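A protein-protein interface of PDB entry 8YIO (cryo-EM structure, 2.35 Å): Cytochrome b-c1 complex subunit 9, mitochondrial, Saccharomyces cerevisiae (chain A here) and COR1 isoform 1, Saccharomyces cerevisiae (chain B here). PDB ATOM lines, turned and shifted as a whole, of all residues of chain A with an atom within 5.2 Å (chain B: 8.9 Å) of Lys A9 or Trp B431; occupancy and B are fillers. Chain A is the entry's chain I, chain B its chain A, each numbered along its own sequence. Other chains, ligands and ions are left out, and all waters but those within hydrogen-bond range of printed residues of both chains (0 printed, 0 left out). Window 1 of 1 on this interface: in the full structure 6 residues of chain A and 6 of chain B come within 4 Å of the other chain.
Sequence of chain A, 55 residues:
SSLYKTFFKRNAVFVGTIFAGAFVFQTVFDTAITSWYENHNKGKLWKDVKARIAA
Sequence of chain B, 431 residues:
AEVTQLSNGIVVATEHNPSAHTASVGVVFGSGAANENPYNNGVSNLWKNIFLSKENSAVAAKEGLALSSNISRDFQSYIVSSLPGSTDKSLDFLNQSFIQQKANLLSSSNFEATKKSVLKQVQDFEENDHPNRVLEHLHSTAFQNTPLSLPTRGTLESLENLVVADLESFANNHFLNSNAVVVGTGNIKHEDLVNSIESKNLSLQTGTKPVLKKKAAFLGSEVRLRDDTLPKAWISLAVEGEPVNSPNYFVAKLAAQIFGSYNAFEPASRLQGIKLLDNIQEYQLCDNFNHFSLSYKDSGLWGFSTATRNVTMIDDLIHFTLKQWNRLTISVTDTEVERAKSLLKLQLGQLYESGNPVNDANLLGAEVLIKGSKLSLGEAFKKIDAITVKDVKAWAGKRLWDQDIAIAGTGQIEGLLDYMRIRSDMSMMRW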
ATOM      1  N   TYR A   4       8.183 -18.475 -12.421  1.00  0.00           N
ATOM      2  CA  TYR A   4       7.565 -19.477 -11.558  1.00  0.00           C
ATOM      3  C   TYR A   4       8.222 -19.450 -10.185  1.00  0.00           C
ATOM      4  O   TYR A   4       7.535 -19.390  -9.159  1.00  0.00           O
ATOM      5  CB  TYR A   4       7.646 -20.888 -12.159  1.00  0.00           C
ATOM      6  CG  TYR A   4       7.446 -21.991 -11.116  1.00  0.00           C
ATOM      7  CD1 TYR A   4       6.268 -22.075 -10.362  1.00  0.00           C
ATOM      8  CD2 TYR A   4       8.439 -22.937 -10.873  1.00  0.00           C
ATOM      9  CE1 TYR A   4       6.102 -23.054  -9.391  1.00  0.00           C
ATOM     10  CE2 TYR A   4       8.267 -23.933  -9.910  1.00  0.00           C
ATOM     11  CZ  TYR A   4       7.095 -23.986  -9.182  1.00  0.00           C
ATOM     12  OH  TYR A   4       6.919 -24.966  -8.231  1.00  0.00           O
ATOM     13  N   LYS A   5       9.555 -19.477 -10.147  1.00  0.00           N
ATOM     14  CA  LYS A   5      10.234 -19.664  -8.874  1.00  0.00           C
ATOM     15  C   LYS A   5      10.295 -18.388  -8.047  1.00  0.00           C
ATOM     16  O   LYS A   5      10.732 -18.436  -6.893  1.00  0.00           O
ATOM     17  CB  LYS A   5      11.633 -20.238  -9.097  1.00  0.00           C
ATOM     18  CG  LYS A   5      11.624 -21.766  -9.073  1.00  0.00           C
ATOM     19  CD  LYS A   5      12.994 -22.368  -8.808  1.00  0.00           C
ATOM     20  CE  LYS A   5      12.850 -23.830  -8.380  1.00  0.00           C
ATOM     21  NZ  LYS A   5      13.879 -24.264  -7.394  1.00  0.00           N
ATOM     22  N   PHE A   7       7.328 -16.500  -7.858  1.00  0.00           N
ATOM     23  CA  PHE A   7       5.925 -16.242  -7.542  1.00  0.00           C
ATOM     24  C   PHE A   7       5.182 -17.429  -6.948  1.00  0.00           C
ATOM     25  O   PHE A   7       4.353 -17.237  -6.058  1.00  0.00           O
ATOM     26  CB  PHE A   7       5.167 -15.771  -8.792  1.00  0.00           C
ATOM     27  CG  PHE A   7       5.235 -14.288  -9.024  1.00  0.00           C
ATOM     28  CD1 PHE A   7       6.415 -13.695  -9.445  1.00  0.00           C
ATOM     29  CD2 PHE A   7       4.114 -13.488  -8.836  1.00  0.00           C
ATOM     30  CE1 PHE A   7       6.483 -12.329  -9.664  1.00  0.00           C
ATOM     31  CE2 PHE A   7       4.175 -12.118  -9.052  1.00  0.00           C
ATOM     32  CZ  PHE A   7       5.362 -11.542  -9.469  1.00  0.00           C
ATOM     33  N   PHE A   8       5.431 -18.657  -7.419  1.00  0.00           N
ATOM     34  CA  PHE A   8       4.617 -19.795  -7.006  1.00  0.00           C
ATOM     35  C   PHE A   8       5.400 -20.997  -6.494  1.00  0.00           C
ATOM     36  O   PHE A   8       4.778 -21.990  -6.101  1.00  0.00           O
ATOM     37  CB  PHE A   8       3.713 -20.254  -8.162  1.00  0.00           C
ATOM     38  CG  PHE A   8       2.956 -19.136  -8.822  1.00  0.00           C
ATOM     39  CD1 PHE A   8       2.051 -18.374  -8.097  1.00  0.00           C
ATOM     40  CD2 PHE A   8       3.145 -18.851 -10.167  1.00  0.00           C
ATOM     41  CE1 PHE A   8       1.351 -17.341  -8.698  1.00  0.00           C
ATOM     42  CE2 PHE A   8       2.448 -17.821 -10.776  1.00  0.00           C
ATOM     43  CZ  PHE A   8       1.550 -17.066 -10.040  1.00  0.00           C
ATOM     44  N   LYS A   9       6.733 -20.953  -6.495  1.00  0.00           N
ATOM     45  CA  LYS A   9       7.497 -22.068  -5.940  1.00  0.00           C
ATOM     46  C   LYS A   9       7.508 -22.018  -4.423  1.00  0.00           C
ATOM     47  O   LYS A   9       7.153 -22.999  -3.756  1.00  0.00           O
ATOM     48  CB  LYS A   9       8.927 -22.055  -6.485  1.00  0.00           C
ATOM     49  CG  LYS A   9       9.850 -23.197  -6.038  1.00  0.00           C
ATOM     50  CD  LYS A   9      10.812 -22.808  -4.894  1.00  0.00           C
ATOM     51  CE  LYS A   9      11.773 -23.943  -4.580  1.00  0.00           C
ATOM     52  NZ  LYS A   9      12.664 -23.648  -3.432  1.00  0.00           N
ATOM     53  N   ARG A  10       7.935 -20.893  -3.864  1.00  0.00           N
ATOM     54  CA  ARG A  10       8.169 -20.788  -2.430  1.00  0.00           C
ATOM     55  C   ARG A  10       6.824 -20.732  -1.731  1.00  0.00           C
ATOM     56  O   ARG A  10       6.183 -19.683  -1.651  1.00  0.00           O
ATOM     57  CB  ARG A  10       9.048 -19.584  -2.121  1.00  0.00           C
ATOM     58  CG  ARG A  10      10.517 -19.971  -2.239  1.00  0.00           C
ATOM     59  CD  ARG A  10      11.469 -19.068  -1.456  1.00  0.00           C
ATOM     60  NE  ARG A  10      12.802 -19.653  -1.255  1.00  0.00           N
ATOM     61  CZ  ARG A  10      13.697 -19.961  -2.199  1.00  0.00           C
ATOM     62  NH1 ARG A  10      13.484 -19.692  -3.482  1.00  0.00           N
ATOM     63  NH2 ARG A  10      14.857 -20.504  -1.840  1.00  0.00           N
ATOM     64  N   ASN A  11       6.395 -21.889  -1.233  1.00  0.00           N
ATOM     65  CA  ASN A  11       5.061 -22.097  -0.696  1.00  0.00           C
ATOM     66  C   ASN A  11       5.000 -21.810   0.799  1.00  0.00           C
ATOM     67  O   ASN A  11       4.097 -22.283   1.498  1.00  0.00           O
ATOM     68  CB  ASN A  11       4.610 -23.521  -1.020  1.00  0.00           C
ATOM     69  CG  ASN A  11       3.164 -23.600  -1.457  1.00  0.00           C
ATOM     70  OD1 ASN A  11       2.288 -22.962  -0.877  1.00  0.00           O
ATOM     71  ND2 ASN A  11       2.911 -24.365  -2.511  1.00  0.00           N
ATOM     72  N   ALA A  12       5.976 -21.054   1.298  1.00  0.00           N
ATOM     73  CA  ALA A  12       5.815 -20.261   2.499  1.00  0.00           C
ATOM     74  C   ALA A  12       5.104 -18.949   2.212  1.00  0.00           C
ATOM     75  O   ALA A  12       4.511 -18.373   3.125  1.00  0.00           O
ATOM     76  CB  ALA A  12       7.178 -19.971   3.139  1.00  0.00           C
ATOM     77  N   ASN B 326      13.484 -34.469  -2.593  1.00  0.00           N
ATOM     78  CA  ASN B 326      13.210 -33.056  -2.338  1.00  0.00           C
ATOM     79  C   ASN B 326      14.274 -32.417  -1.460  1.00  0.00           C
ATOM     80  O   ASN B 326      14.490 -31.204  -1.532  1.00  0.00           O
ATOM     81  CB  ASN B 326      11.814 -32.884  -1.736  1.00  0.00           C
ATOM     82  CG  ASN B 326      10.703 -33.140  -2.731  1.00  0.00           C
ATOM     83  OD1 ASN B 326      10.912 -33.054  -3.934  1.00  0.00           O
ATOM     84  ND2 ASN B 326       9.518 -33.456  -2.236  1.00  0.00           N
ATOM     85  N   ARG B 327      14.953 -33.212  -0.629  1.00  0.00           N
ATOM     86  CA  ARG B 327      15.939 -32.679   0.299  1.00  0.00           C
ATOM     87  C   ARG B 327      17.223 -32.233  -0.387  1.00  0.00           C
ATOM     88  O   ARG B 327      17.994 -31.483   0.214  1.00  0.00           O
ATOM     89  CB  ARG B 327      16.263 -33.720   1.368  1.00  0.00           C
ATOM     90  CG  ARG B 327      15.076 -34.109   2.226  1.00  0.00           C
ATOM     91  CD  ARG B 327      15.478 -35.078   3.321  1.00  0.00           C
ATOM     92  NE  ARG B 327      16.555 -34.544   4.145  1.00  0.00           N
ATOM     93  CZ  ARG B 327      17.743 -35.117   4.296  1.00  0.00           C
ATOM     94  NH1 ARG B 327      18.659 -34.547   5.060  1.00  0.00           N
ATOM     95  NH2 ARG B 327      18.017 -36.257   3.681  1.00  0.00           N
ATOM     96  N   THR B 329      17.353 -30.207  -2.853  1.00  0.00           N
ATOM     97  CA  THR B 329      17.151 -28.784  -3.085  1.00  0.00           C
ATOM     98  C   THR B 329      17.121 -28.002  -1.778  1.00  0.00           C
ATOM     99  O   THR B 329      17.611 -26.871  -1.716  1.00  0.00           O
ATOM    100  CB  THR B 329      15.848 -28.571  -3.868  1.00  0.00           C
ATOM    101  OG1 THR B 329      15.854 -29.402  -5.032  1.00  0.00           O
ATOM    102  CG2 THR B 329      15.681 -27.122  -4.308  1.00  0.00           C
ATOM    103  N   ILE B 330      16.595 -28.604  -0.715  1.00  0.00           N
ATOM    104  CA  ILE B 330      16.276 -27.864   0.497  1.00  0.00           C
ATOM    105  C   ILE B 330      17.321 -28.065   1.593  1.00  0.00           C
ATOM    106  O   ILE B 330      17.934 -27.095   2.047  1.00  0.00           O
ATOM    107  CB  ILE B 330      14.865 -28.240   0.988  1.00  0.00           C
ATOM    108  CG1 ILE B 330      13.820 -27.725   0.000  1.00  0.00           C
ATOM    109  CG2 ILE B 330      14.595 -27.670   2.368  1.00  0.00           C
ATOM    110  CD1 ILE B 330      12.390 -27.987   0.411  1.00  0.00           C
ATOM    111  N   SER B 331      17.531 -29.305   2.040  1.00  0.00           N
ATOM    112  CA  SER B 331      18.200 -29.521   3.321  1.00  0.00           C
ATOM    113  C   SER B 331      19.195 -30.679   3.281  1.00  0.00           C
ATOM    114  O   SER B 331      19.224 -31.512   4.191  1.00  0.00           O
ATOM    115  CB  SER B 331      17.174 -29.768   4.425  1.00  0.00           C
ATOM    116  OG  SER B 331      16.460 -30.963   4.178  1.00  0.00           O
ATOM    117  N   VAL B 332      20.027 -30.760   2.251  1.00  0.00           N
ATOM    118  CA  VAL B 332      21.071 -31.782   2.222  1.00  0.00           C
ATOM    119  C   VAL B 332      22.236 -31.326   3.106  1.00  0.00           C
ATOM    120  O   VAL B 332      22.619 -30.151   3.099  1.00  0.00           O
ATOM    121  CB  VAL B 332      21.501 -32.085   0.771  1.00  0.00           C
ATOM    122  CG1 VAL B 332      21.995 -30.838   0.030  1.00  0.00           C
ATOM    123  CG2 VAL B 332      22.535 -33.201   0.721  1.00  0.00           C
ATOM    124  N   LYS B 393      22.840 -28.295  -4.415  1.00  0.00           N
ATOM    125  CA  LYS B 393      21.556 -27.604  -4.324  1.00  0.00           C
ATOM    126  C   LYS B 393      21.213 -26.856  -5.605  1.00  0.00           C
ATOM    127  O   LYS B 393      20.034 -26.742  -5.953  1.00  0.00           O
ATOM    128  CB  LYS B 393      21.564 -26.638  -3.142  1.00  0.00           C
ATOM    129  CG  LYS B 393      21.328 -27.295  -1.803  1.00  0.00           C
ATOM    130  CD  LYS B 393      21.397 -26.290  -0.677  1.00  0.00           C
ATOM    131  CE  LYS B 393      21.019 -26.923   0.646  1.00  0.00           C
ATOM    132  NZ  LYS B 393      21.067 -25.949   1.762  1.00  0.00           N
ATOM    133  N   ALA B 396      20.122 -29.639  -8.265  1.00  0.00           N
ATOM    134  CA  ALA B 396      18.833 -30.269  -8.013  1.00  0.00           C
ATOM    135  C   ALA B 396      17.673 -29.303  -8.193  1.00  0.00           C
ATOM    136  O   ALA B 396      16.562 -29.735  -8.512  1.00  0.00           O
ATOM    137  CB  ALA B 396      18.803 -30.870  -6.609  1.00  0.00           C
ATOM    138  N   GLY B 397      17.905 -28.003  -7.996  1.00  0.00           N
ATOM    139  CA  GLY B 397      16.885 -27.010  -8.280  1.00  0.00           C
ATOM    140  C   GLY B 397      16.562 -26.873  -9.751  1.00  0.00           C
ATOM    141  O   GLY B 397      15.468 -26.418 -10.095  1.00  0.00           O
ATOM    142  N   TRP B 401      13.536 -30.346  -9.028  1.00  0.00           N
ATOM    143  CA  TRP B 401      12.415 -29.657  -8.397  1.00  0.00           C
ATOM    144  C   TRP B 401      11.360 -29.270  -9.433  1.00  0.00           C
ATOM    145  O   TRP B 401      11.641 -28.492 -10.350  1.00  0.00           O
ATOM    146  CB  TRP B 401      12.917 -28.426  -7.644  1.00  0.00           C
ATOM    147  CG  TRP B 401      11.876 -27.797  -6.766  1.00  0.00           C
ATOM    148  CD1 TRP B 401      11.005 -26.813  -7.116  1.00  0.00           C
ATOM    149  CD2 TRP B 401      11.595 -28.113  -5.396  1.00  0.00           C
ATOM    150  NE1 TRP B 401      10.194 -26.501  -6.059  1.00  0.00           N
ATOM    151  CE2 TRP B 401      10.540 -27.276  -4.986  1.00  0.00           C
ATOM    152  CE3 TRP B 401      12.132 -29.020  -4.478  1.00  0.00           C
ATOM    153  CZ2 TRP B 401      10.007 -27.319  -3.700  1.00  0.00           C
ATOM    154  CZ3 TRP B 401      11.604 -29.059  -3.198  1.00  0.00           C
ATOM    155  CH2 TRP B 401      10.552 -28.213  -2.822  1.00  0.00           C
ATOM    156  N   ASP B 402      10.158 -29.844  -9.278  1.00  0.00           N
ATOM    157  CA  ASP B 402       8.970 -29.578 -10.106  1.00  0.00           C
ATOM    158  C   ASP B 402       9.199 -29.899 -11.586  1.00  0.00           C
ATOM    159  O   ASP B 402       8.920 -29.089 -12.467  1.00  0.00           O
ATOM    160  CB  ASP B 402       8.485 -28.136  -9.923  1.00  0.00           C
ATOM    161  CG  ASP B 402       7.002 -27.985 -10.168  1.00  0.00           C
ATOM    162  OD1 ASP B 402       6.211 -28.670  -9.493  1.00  0.00           O
ATOM    163  OD2 ASP B 402       6.625 -27.177 -11.035  1.00  0.00           O
ATOM    164  N   MET B 426       6.942 -34.331  -6.735  1.00  0.00           N
ATOM    165  CA  MET B 426       8.227 -33.765  -7.123  1.00  0.00           C
ATOM    166  C   MET B 426       8.462 -32.378  -6.542  1.00  0.00           C
ATOM    167  O   MET B 426       9.546 -31.822  -6.733  1.00  0.00           O
ATOM    168  CB  MET B 426       8.344 -33.718  -8.649  1.00  0.00           C
ATOM    169  CG  MET B 426       8.294 -35.080  -9.319  1.00  0.00           C
ATOM    170  SD  MET B 426       9.584 -36.211  -8.769  1.00  0.00           S
ATOM    171  CE  MET B 426      11.016 -35.536  -9.590  1.00  0.00           C
ATOM    172  N   SER B 427       7.480 -31.808  -5.853  1.00  0.00           N
ATOM    173  CA  SER B 427       7.666 -30.616  -5.043  1.00  0.00           C
ATOM    174  C   SER B 427       7.033 -30.830  -3.681  1.00  0.00           C
ATOM    175  O   SER B 427       6.114 -31.634  -3.516  1.00  0.00           O
ATOM    176  CB  SER B 427       7.045 -29.363  -5.679  1.00  0.00           C
ATOM    177  OG  SER B 427       7.738 -28.970  -6.841  1.00  0.00           O
ATOM    178  N   MET B 428       7.546 -30.102  -2.702  1.00  0.00           N
ATOM    179  CA  MET B 428       6.828 -29.873  -1.462  1.00  0.00           C
ATOM    180  C   MET B 428       6.098 -28.545  -1.554  1.00  0.00           C
ATOM    181  O   MET B 428       6.622 -27.564  -2.088  1.00  0.00           O
ATOM    182  CB  MET B 428       7.766 -29.861  -0.250  1.00  0.00           C
ATOM    183  CG  MET B 428       8.635 -31.084  -0.099  1.00  0.00           C
ATOM    184  SD  MET B 428      10.116 -30.808   0.885  1.00  0.00           S
ATOM    185  CE  MET B 428       9.420 -30.244   2.431  1.00  0.00           C
ATOM    186  N   MET B 429       4.882 -28.513  -1.017  1.00  0.00           N
ATOM    187  CA  MET B 429       4.205 -27.235  -0.831  1.00  0.00           C
ATOM    188  C   MET B 429       4.547 -26.599   0.513  1.00  0.00           C
ATOM    189  O   MET B 429       3.727 -25.867   1.080  1.00  0.00           O
ATOM    190  CB  MET B 429       2.691 -27.390  -1.030  1.00  0.00           C
ATOM    191  CG  MET B 429       1.933 -28.277  -0.065  1.00  0.00           C
ATOM    192  SD  MET B 429       0.181 -28.158  -0.471  1.00  0.00           S
ATOM    193  CE  MET B 429      -0.281 -26.702   0.462  1.00  0.00           C
ATOM    194  N   ARG B 430       5.752 -26.859   1.015  1.00  0.00           N
ATOM    195  CA  ARG B 430       6.333 -26.231   2.188  1.00  0.00           C
ATOM    196  C   ARG B 430       7.322 -25.137   1.790  1.00  0.00           C
ATOM    197  O   ARG B 430       7.222 -24.005   2.275  1.00  0.00           O
ATOM    198  CB  ARG B 430       7.001 -27.282   3.096  1.00  0.00           C
ATOM    199  CG  ARG B 430       6.063 -28.355   3.719  1.00  0.00           C
ATOM    200  CD  ARG B 430       5.760 -29.541   2.799  1.00  0.00           C
ATOM    201  NE  ARG B 430       4.588 -30.315   3.193  1.00  0.00           N
ATOM    202  CZ  ARG B 430       4.018 -31.230   2.417  1.00  0.00           C
ATOM    203  NH1 ARG B 430       4.510 -31.478   1.211  1.00  0.00           N
ATOM    204  NH2 ARG B 430       2.952 -31.894   2.838  1.00  0.00           N
ATOM    205  N   TRP B 431       8.268 -25.447   0.904  1.00  0.00           N
ATOM    206  CA  TRP B 431       9.105 -24.407   0.312  1.00  0.00           C
ATOM    207  C   TRP B 431       8.746 -24.206  -1.152  1.00  0.00           C
ATOM    208  O   TRP B 431       9.615 -23.931  -1.980  1.00  0.00           O
ATOM    209  CB  TRP B 431      10.600 -24.729   0.414  1.00  0.00           C
ATOM    210  CG  TRP B 431      11.194 -24.719   1.796  1.00  0.00           C
ATOM    211  CD1 TRP B 431      10.540 -24.871   2.986  1.00  0.00           C
ATOM    212  CD2 TRP B 431      12.567 -24.476   2.125  1.00  0.00           C
ATOM    213  NE1 TRP B 431      11.428 -24.781   4.030  1.00  0.00           N
ATOM    214  CE2 TRP B 431      12.678 -24.533   3.530  1.00  0.00           C
ATOM    215  CE3 TRP B 431      13.716 -24.231   1.368  1.00  0.00           C
ATOM    216  CZ2 TRP B 431      13.889 -24.351   4.190  1.00  0.00           C
ATOM    217  CZ3 TRP B 431      14.921 -24.048   2.026  1.00  0.00           C
ATOM    218  CH2 TRP B 431      15.000 -24.115   3.422  1.00  0.00           C
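Among the printed residues, merely in contact across the chains: Asn A11 with Met B429 (3.3 Å), Asn A11 with Trp B431 (3.3 Å), Lys A9 with Trp B401 (3.3 Å), Asn A11 with Arg B430 (3.5 Å), Arg A10 with Trp B431 (3.5 Å), Tyr A4 with Asp B402 (3.6 Å), Lys A5 with Trp B401 (3.7 Å) and Lys A5 with Gly B397 (3.8 Å).
Of the 8 printed residues of chain A, 6 touch a printed residue of chain B. Hydrophobic or aromatic side chains of chain A within 4 Å of the printed part of chain B: Tyr A4. Of the 17 printed residues of chain B, 6 touch a printed residue of chain A. Hydrophobic or aromatic side chains of chain B within 4 Å of the printed part of chain A: Trp B401 and Met B429. Among the printed residues, 10 pairs touch across the chains. Among the printed residues, no Asp or Glu carboxylate lies within 4 Å of a Lys or Arg side-chain nitrogen of the other chain.
Lys A9 touches two residues of chain B. Trp B431 touches just these residues of chain A: Lys A9, Arg A10 and Asn A11. Lys A5 touches just these residues of chain B: Gly B397 (3.8 Å) and Trp B401 (3.7 Å). Of the printed residues of chain A, Arg B430 touches Asn A11 (3.5 Å) and Ala A12 (3.3 Å). Of the printed residues of chain A, Trp B401 touches Lys A5 (3.7 Å) and Lys A9 (3.3 Å). Printed residues of chain A within 4 Å of Met B429: Asn A11 (3.3 Å). Ser B427 touches none of the printed residues of chain A. Asn B326 touches none of the printed residues of chain A. The nearest residue of chain B that does not touch Lys A9 is Thr B329 (4.7 Å). The nearest printed residue of chain B that does not touch Ala A12 is Trp B431 (4.7 Å).
The side-chain amino group (NZ) of Lys A9 lies close to the backbone carbonyl oxygen (O) of Trp B431 (3.4 Å). The backbone carbonyl oxygen (O) of Arg B430 is in hydrogen-bond range of the backbone NH (N) of Ala A12.
N of Lys A9 lies within hydrogen-bond range of O of Tyr A4 (3.2 Å). O of Ala B396 lies within hydrogen-bond range of N of Trp B401 (3.1 Å). N of Asp B402 sits at hydrogen-bond distance from O of Met B426 (3.3 Å). The side-chain carboxylate of Asp B402 sits at hydrogen-bond distance from the side-chain hydroxyl of Ser B427, 3.1 Å away.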
